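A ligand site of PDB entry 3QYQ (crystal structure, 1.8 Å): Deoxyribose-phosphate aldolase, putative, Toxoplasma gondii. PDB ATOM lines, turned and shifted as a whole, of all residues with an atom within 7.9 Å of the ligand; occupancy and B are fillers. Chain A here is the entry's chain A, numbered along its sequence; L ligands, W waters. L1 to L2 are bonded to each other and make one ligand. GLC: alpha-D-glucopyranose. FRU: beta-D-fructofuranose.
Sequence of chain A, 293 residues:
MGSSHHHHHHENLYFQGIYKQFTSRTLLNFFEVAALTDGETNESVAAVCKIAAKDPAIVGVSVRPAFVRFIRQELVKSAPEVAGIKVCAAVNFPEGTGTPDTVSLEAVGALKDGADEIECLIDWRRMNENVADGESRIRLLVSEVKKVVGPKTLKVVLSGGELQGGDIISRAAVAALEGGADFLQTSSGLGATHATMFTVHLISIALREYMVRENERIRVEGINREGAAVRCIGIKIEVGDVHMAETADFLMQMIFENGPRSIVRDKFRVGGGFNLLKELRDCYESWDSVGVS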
ATOM      1  N   VAL A  33      23.283  -7.891  21.191  1.00  0.00           N
ATOM      2  CA  VAL A  33      23.518  -8.203  22.587  1.00  0.00           C
ATOM      3  C   VAL A  33      22.733  -9.435  23.009  1.00  0.00           C
ATOM      4  O   VAL A  33      21.549  -9.587  22.727  1.00  0.00           O
ATOM      5  CB  VAL A  33      23.248  -6.959  23.502  1.00  0.00           C
ATOM      6  CG1 VAL A  33      21.775  -6.560  23.544  1.00  0.00           C
ATOM      7  CG2 VAL A  33      23.737  -7.211  24.914  1.00  0.00           C
ATOM      8  N   ALA A  34      23.443 -10.336  23.665  1.00  0.00           N
ATOM      9  CA  ALA A  34      22.864 -11.581  24.152  1.00  0.00           C
ATOM     10  C   ALA A  34      22.293 -11.400  25.549  1.00  0.00           C
ATOM     11  O   ALA A  34      22.936 -10.821  26.407  1.00  0.00           O
ATOM     12  CB  ALA A  34      23.950 -12.651  24.187  1.00  0.00           C
ATOM     13  N   ALA A  35      21.052 -11.844  25.737  1.00  0.00           N
ATOM     14  CA  ALA A  35      20.386 -11.805  27.045  1.00  0.00           C
ATOM     15  C   ALA A  35      19.715 -13.172  27.118  1.00  0.00           C
ATOM     16  O   ALA A  35      18.492 -13.287  27.093  1.00  0.00           O
ATOM     17  CB  ALA A  35      19.359 -10.689  27.106  1.00  0.00           C
ATOM     18  N   LEU A  36      20.542 -14.218  27.229  1.00  0.00           N
ATOM     19  CA  LEU A  36      20.094 -15.604  27.227  1.00  0.00           C
ATOM     20  C   LEU A  36      20.331 -16.427  28.492  1.00  0.00           C
ATOM     21  O   LEU A  36      20.067 -17.629  28.495  1.00  0.00           O
ATOM     22  CB  LEU A  36      20.895 -16.299  26.108  1.00  0.00           C
ATOM     23  CG  LEU A  36      20.714 -15.796  24.674  1.00  0.00           C
ATOM     24  CD1 LEU A  36      21.850 -16.289  23.786  1.00  0.00           C
ATOM     25  CD2 LEU A  36      19.320 -16.182  24.135  1.00  0.00           C
ATOM     26  N   THR A  37      20.826 -15.807  29.560  1.00  0.00           N
ATOM     27  CA  THR A  37      21.126 -16.556  30.778  1.00  0.00           C
ATOM     28  C   THR A  37      19.886 -17.182  31.418  1.00  0.00           C
ATOM     29  O   THR A  37      18.776 -16.686  31.235  1.00  0.00           O
ATOM     30  CB  THR A  37      21.824 -15.658  31.820  1.00  0.00           C
ATOM     31  OG1 THR A  37      20.910 -14.672  32.294  1.00  0.00           O
ATOM     32  CG2 THR A  37      23.052 -14.992  31.213  1.00  0.00           C
ATOM     33  N   ASP A  38      20.085 -18.282  32.125  1.00  0.00           N
ATOM     34  CA  ASP A  38      18.977 -18.980  32.795  1.00  0.00           C
ATOM     35  C   ASP A  38      18.227 -18.030  33.736  1.00  0.00           C
ATOM     36  O   ASP A  38      17.019 -18.175  33.939  1.00  0.00           O
ATOM     37  CB  ASP A  38      19.477 -20.141  33.660  1.00  0.00           C
ATOM     38  CG  ASP A  38      20.117 -21.270  32.858  1.00  0.00           C
ATOM     39  OD1 ASP A  38      20.135 -21.237  31.609  1.00  0.00           O
ATOM     40  OD2 ASP A  38      20.599 -22.233  33.519  1.00  0.00           O
ATOM     41  N   GLY A  39      18.937 -17.074  34.330  1.00  0.00           N
ATOM     42  CA  GLY A  39      18.336 -16.144  35.276  1.00  0.00           C
ATOM     43  C   GLY A  39      17.589 -14.942  34.737  1.00  0.00           C
ATOM     44  O   GLY A  39      17.149 -14.089  35.534  1.00  0.00           O
ATOM     45  N   GLU A  40      17.409 -14.841  33.420  1.00  0.00           N
ATOM     46  CA  GLU A  40      16.722 -13.686  32.865  1.00  0.00           C
ATOM     47  C   GLU A  40      15.261 -13.576  33.328  1.00  0.00           C
ATOM     48  O   GLU A  40      14.569 -14.575  33.517  1.00  0.00           O
ATOM     49  CB  GLU A  40      16.733 -13.714  31.326  1.00  0.00           C
ATOM     50  CG  GLU A  40      18.111 -13.745  30.658  1.00  0.00           C
ATOM     51  CD  GLU A  40      18.947 -12.484  30.815  1.00  0.00           C
ATOM     52  OE1 GLU A  40      18.510 -11.513  31.469  1.00  0.00           O
ATOM     53  OE2 GLU A  40      20.059 -12.456  30.228  1.00  0.00           O
ATOM     54  N   THR A  41      14.833 -12.334  33.508  1.00  0.00           N
ATOM     55  CA  THR A  41      13.479 -12.001  33.913  1.00  0.00           C
ATOM     56  C   THR A  41      13.061 -10.901  32.962  1.00  0.00           C
ATOM     57  O   THR A  41      13.898 -10.362  32.238  1.00  0.00           O
ATOM     58  CB  THR A  41      13.447 -11.468  35.334  1.00  0.00           C
ATOM     59  OG1 THR A  41      14.270 -10.291  35.413  1.00  0.00           O
ATOM     60  CG2 THR A  41      13.948 -12.510  36.298  1.00  0.00           C
ATOM     61  N   ASN A  42      11.775 -10.551  32.932  1.00  0.00           N
ATOM     62  CA  ASN A  42      11.355  -9.457  32.056  1.00  0.00           C
ATOM     63  C   ASN A  42      12.117  -8.184  32.398  1.00  0.00           C
ATOM     64  O   ASN A  42      12.491  -7.433  31.504  1.00  0.00           O
ATOM     65  CB  ASN A  42       9.854  -9.186  32.153  1.00  0.00           C
ATOM     66  CG  ASN A  42       9.022 -10.280  31.562  1.00  0.00           C
ATOM     67  OD1 ASN A  42       9.529 -11.193  30.918  1.00  0.00           O
ATOM     68  ND2 ASN A  42       7.708 -10.191  31.764  1.00  0.00           N
ATOM     69  N   GLU A  43      12.351  -7.955  33.683  1.00  0.00           N
ATOM     70  CA  GLU A  43      13.081  -6.764  34.122  1.00  0.00           C
ATOM     71  C   GLU A  43      14.520  -6.730  33.652  1.00  0.00           C
ATOM     72  O   GLU A  43      14.984  -5.685  33.177  1.00  0.00           O
ATOM     73  CB  GLU A  43      13.021  -6.616  35.647  1.00  0.00           C
ATOM     74  CG  GLU A  43      11.632  -6.311  36.168  1.00  0.00           C
ATOM     75  CD  GLU A  43      11.071  -5.007  35.630  1.00  0.00           C
ATOM     76  OE1 GLU A  43      11.828  -4.247  34.972  1.00  0.00           O
ATOM     77  OE2 GLU A  43       9.874  -4.743  35.858  1.00  0.00           O
ATOM     78  N   SER A  44      15.248  -7.836  33.767  1.00  0.00           N
ATOM     79  CA  SER A  44      16.633  -7.869  33.334  1.00  0.00           C
ATOM     80  C   SER A  44      16.719  -7.706  31.824  1.00  0.00           C
ATOM     81  O   SER A  44      17.593  -7.009  31.318  1.00  0.00           O
ATOM     82  CB  SER A  44      17.342  -9.153  33.775  1.00  0.00           C
ATOM     83  OG  SER A  44      16.746 -10.288  33.178  1.00  0.00           O
ATOM     84  N   VAL A  45      15.789  -8.331  31.100  1.00  0.00           N
ATOM     85  CA  VAL A  45      15.740  -8.243  29.644  1.00  0.00           C
ATOM     86  C   VAL A  45      15.416  -6.813  29.205  1.00  0.00           C
ATOM     87  O   VAL A  45      16.004  -6.292  28.243  1.00  0.00           O
ATOM     88  CB  VAL A  45      14.717  -9.237  29.048  1.00  0.00           C
ATOM     89  CG1 VAL A  45      14.472  -8.983  27.562  1.00  0.00           C
ATOM     90  CG2 VAL A  45      15.183 -10.664  29.318  1.00  0.00           C
ATOM     91  N   ALA A  46      14.494  -6.175  29.921  1.00  0.00           N
ATOM     92  CA  ALA A  46      14.110  -4.804  29.619  1.00  0.00           C
ATOM     93  C   ALA A  46      15.312  -3.884  29.752  1.00  0.00           C
ATOM     94  O   ALA A  46      15.490  -2.989  28.935  1.00  0.00           O
ATOM     95  CB  ALA A  46      12.965  -4.352  30.534  1.00  0.00           C
ATOM     96  N   ALA A  47      16.150  -4.111  30.758  1.00  0.00           N
ATOM     97  CA  ALA A  47      17.327  -3.268  30.978  1.00  0.00           C
ATOM     98  C   ALA A  47      18.286  -3.345  29.783  1.00  0.00           C
ATOM     99  O   ALA A  47      18.815  -2.314  29.356  1.00  0.00           O
ATOM    100  CB  ALA A  47      18.046  -3.672  32.257  1.00  0.00           C
ATOM    101  N   VAL A  48      18.492  -4.544  29.270  1.00  0.00           N
ATOM    102  CA  VAL A  48      19.387  -4.769  28.131  1.00  0.00           C
ATOM    103  C   VAL A  48      18.815  -4.114  26.873  1.00  0.00           C
ATOM    104  O   VAL A  48      19.538  -3.436  26.142  1.00  0.00           O
ATOM    105  CB  VAL A  48      19.610  -6.270  27.885  1.00  0.00           C
ATOM    106  CG1 VAL A  48      20.411  -6.493  26.588  1.00  0.00           C
ATOM    107  CG2 VAL A  48      20.306  -6.905  29.067  1.00  0.00           C
ATOM    108  N   CYS A  49      17.520  -4.318  26.629  1.00  0.00           N
ATOM    109  CA  CYS A  49      16.888  -3.719  25.450  1.00  0.00           C
ATOM    110  C   CYS A  49      16.983  -2.203  25.420  1.00  0.00           C
ATOM    111  O   CYS A  49      17.157  -1.618  24.357  1.00  0.00           O
ATOM    112  CB  CYS A  49      15.413  -4.136  25.338  1.00  0.00           C
ATOM    113  SG  CYS A  49      15.165  -5.869  24.981  1.00  0.00           S
ATOM    114  N   SER A  62      19.383 -10.831  21.406  1.00  0.00           N
ATOM    115  CA  SER A  62      19.141 -12.269  21.288  1.00  0.00           C
ATOM    116  C   SER A  62      18.551 -12.746  22.613  1.00  0.00           C
ATOM    117  O   SER A  62      19.154 -12.556  23.674  1.00  0.00           O
ATOM    118  CB  SER A  62      20.426 -13.053  20.985  1.00  0.00           C
ATOM    119  OG  SER A  62      20.943 -12.714  19.732  1.00  0.00           O
ATOM    120  N   LEU A 190      25.806 -18.027  24.989  1.00  0.00           N
ATOM    121  CA  LEU A 190      25.651 -18.446  26.370  1.00  0.00           C
ATOM    122  C   LEU A 190      26.796 -19.398  26.679  1.00  0.00           C
ATOM    123  O   LEU A 190      27.022 -20.365  25.941  1.00  0.00           O
ATOM    124  CB  LEU A 190      24.318 -19.153  26.607  1.00  0.00           C
ATOM    125  CG  LEU A 190      24.031 -19.507  28.073  1.00  0.00           C
ATOM    126  CD1 LEU A 190      23.958 -18.232  28.900  1.00  0.00           C
ATOM    127  CD2 LEU A 190      22.737 -20.293  28.228  1.00  0.00           C
ATOM    128  N   GLY A 273      28.137  -9.599  25.124  1.00  0.00           N
ATOM    129  CA  GLY A 273      27.376  -9.372  26.327  1.00  0.00           C
ATOM    130  C   GLY A 273      27.018  -7.947  26.628  1.00  0.00           C
ATOM    131  O   GLY A 273      27.435  -7.001  25.958  1.00  0.00           O
ATOM    132  N   PHE A 274      26.245  -7.801  27.696  1.00  0.00           N
ATOM    133  CA  PHE A 274      25.768  -6.522  28.157  1.00  0.00           C
ATOM    134  C   PHE A 274      26.905  -5.618  28.638  1.00  0.00           C
ATOM    135  O   PHE A 274      26.904  -4.433  28.353  1.00  0.00           O
ATOM    136  CB  PHE A 274      24.696  -6.784  29.229  1.00  0.00           C
ATOM    137  CG  PHE A 274      23.981  -5.557  29.712  1.00  0.00           C
ATOM    138  CD1 PHE A 274      23.527  -4.614  28.824  1.00  0.00           C
ATOM    139  CD2 PHE A 274      23.597  -5.459  31.039  1.00  0.00           C
ATOM    140  CE1 PHE A 274      22.817  -3.513  29.262  1.00  0.00           C
ATOM    141  CE2 PHE A 274      22.865  -4.379  31.477  1.00  0.00           C
ATOM    142  CZ  PHE A 274      22.469  -3.409  30.582  1.00  0.00           C
ATOM    143  N   ASN A 275      27.895  -6.174  29.338  1.00  0.00           N
ATOM    144  CA  ASN A 275      29.015  -5.320  29.787  1.00  0.00           C
ATOM    145  C   ASN A 275      29.810  -4.787  28.593  1.00  0.00           C
ATOM    146  O   ASN A 275      30.257  -3.633  28.606  1.00  0.00           O
ATOM    147  CB  ASN A 275      29.910  -6.033  30.800  1.00  0.00           C
ATOM    148  CG  ASN A 275      29.264  -6.143  32.173  1.00  0.00           C
ATOM    149  OD1 ASN A 275      28.454  -5.288  32.561  1.00  0.00           O
ATOM    150  ND2 ASN A 275      29.641  -7.157  32.937  1.00  0.00           N
ATOM    151  N   LEU A 276      29.959  -5.602  27.555  1.00  0.00           N
ATOM    152  CA  LEU A 276      30.697  -5.177  26.363  1.00  0.00           C
ATOM    153  C   LEU A 276      29.898  -4.063  25.672  1.00  0.00           C
ATOM    154  O   LEU A 276      30.482  -3.079  25.204  1.00  0.00           O
ATOM    155  CB  LEU A 276      30.978  -6.347  25.418  1.00  0.00           C
ATOM    156  CG  LEU A 276      31.727  -6.041  24.130  1.00  0.00           C
ATOM    157  CD1 LEU A 276      33.046  -5.320  24.351  1.00  0.00           C
ATOM    158  CD2 LEU A 276      31.943  -7.339  23.301  1.00  0.00           C
ATOM    159  N   LYS A 278      27.902  -1.904  27.065  1.00  0.00           N
ATOM    160  CA  LYS A 278      28.073  -0.688  27.872  1.00  0.00           C
ATOM    161  C   LYS A 278      29.460  -0.065  27.655  1.00  0.00           C
ATOM    162  O   LYS A 278      29.596   1.148  27.590  1.00  0.00           O
ATOM    163  CB  LYS A 278      27.749  -0.966  29.351  1.00  0.00           C
ATOM    164  CG  LYS A 278      26.259  -1.261  29.534  1.00  0.00           C
ATOM    165  CD  LYS A 278      25.812  -1.495  30.973  1.00  0.00           C
ATOM    166  CE  LYS A 278      26.426  -2.722  31.598  1.00  0.00           C
ATOM    167  NZ  LYS A 278      25.865  -2.971  32.975  1.00  0.00           N
HETATM  168  C1  GLC L   1      22.944  -9.542  35.551  1.00  0.00           C
HETATM  169  C2  GLC L   1      23.503 -10.044  36.862  1.00  0.00           C
HETATM  170  C3  GLC L   1      23.163 -11.507  37.027  1.00  0.00           C
HETATM  171  C4  GLC L   1      21.655 -11.694  37.005  1.00  0.00           C
HETATM  172  C5  GLC L   1      21.032 -10.981  35.808  1.00  0.00           C
HETATM  173  C6  GLC L   1      19.560 -10.826  36.075  1.00  0.00           C
HETATM  174  O2  GLC L   1      24.902  -9.862  36.840  1.00  0.00           O
HETATM  175  O3  GLC L   1      23.691 -12.062  38.234  1.00  0.00           O
HETATM  176  O4  GLC L   1      21.370 -13.095  36.951  1.00  0.00           O
HETATM  177  O5  GLC L   1      21.531  -9.676  35.576  1.00  0.00           O
HETATM  178  O6  GLC L   1      19.033 -11.659  35.092  1.00  0.00           O
HETATM  179  C1  FRU L   2      25.082  -8.506  33.626  1.00  0.00           C
HETATM  180  C2  FRU L   2      23.807  -9.288  33.338  1.00  0.00           C
HETATM  181  C3  FRU L   2      23.782 -10.093  32.038  1.00  0.00           C
HETATM  182  C4  FRU L   2      22.284 -10.028  31.763  1.00  0.00           C
HETATM  183  C5  FRU L   2      21.965  -8.590  32.094  1.00  0.00           C
HETATM  184  C6  FRU L   2      20.530  -8.369  32.469  1.00  0.00           C
HETATM  185  O1  FRU L   2      25.711  -8.089  32.450  1.00  0.00           O
HETATM  186  O2  FRU L   2      23.520 -10.180  34.406  1.00  0.00           O
HETATM  187  O3  FRU L   2      24.211 -11.436  32.203  1.00  0.00           O
HETATM  188  O4  FRU L   2      21.842 -10.440  30.494  1.00  0.00           O
HETATM  189  O5  FRU L   2      22.775  -8.338  33.212  1.00  0.00           O
HETATM  190  O6  FRU L   2      20.167  -7.010  32.579  1.00  0.00           O
HETATM  191  O   HOH W   1      25.851  -5.242  33.796  1.00  0.00           O
HETATM  192  O   HOH W   2      23.433  -5.862  35.037  1.00  0.00           O
HETATM  193  O   HOH W   3      20.411 -15.290  38.968  1.00  0.00           O
HETATM  194  O   HOH W   4      28.027  -8.017  35.348  1.00  0.00           O
HETATM  195  O   HOH W   5      24.787 -13.452  34.080  1.00  0.00           O
HETATM  196  O   HOH W   6      23.578 -10.125  28.654  1.00  0.00           O
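Merely in contact with the ligand: Ala 35 (3.98 Å), Thr 37 (3.9 Å), Ala 47 (3.97 Å), Val 48 (3.5 Å), Phe 274 (3.6 Å) and Asn 275 (3.9 Å).
The nearest printed residue that does not touch the ligand is Ala 34 (4.2 Å).
O of Gly 39 is in hydrogen-bond range of O6 of GLC L1 (3.1 Å).
The side-chain hydroxyl (OG) of Ser 44 is in hydrogen-bond range of an oxygen (O6) of GLC L1.
The side-chain carboxylate of Glu 40 sits at hydrogen-bond distance from an oxygen (O4) of FRU L2, 2.7 Å away.
O6 of FRU L2 is in hydrogen-bond range of O of Ser 44 (2.9 Å).
Water W6 bridges O of Ala 34 and O4 of FRU L2.
Water W1 lies within hydrogen-bond range of NZ of Lys 278 (2.4 Å), OD1 of Asn 275 (2.9 Å) and O1 of FRU L2 (3.2 Å).
OE2 of Glu 40 is in hydrogen-bond range of OG1 of Thr 37 (3.1 Å).
OG of Ser 44 lies within hydrogen-bond range of OE1 of Glu 40, 2.7 Å away.
The backbone NH (N) of Ala 35 sits at hydrogen-bond distance from the backbone carbonyl oxygen (O) of Ser 62, 2.9 Å away.
N of Thr 41 sits at hydrogen-bond distance from OG of Ser 44 (2.8 Å).
The side-chain amide oxygen of Asn 275 sits close to the side-chain amino group of Lys 278.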
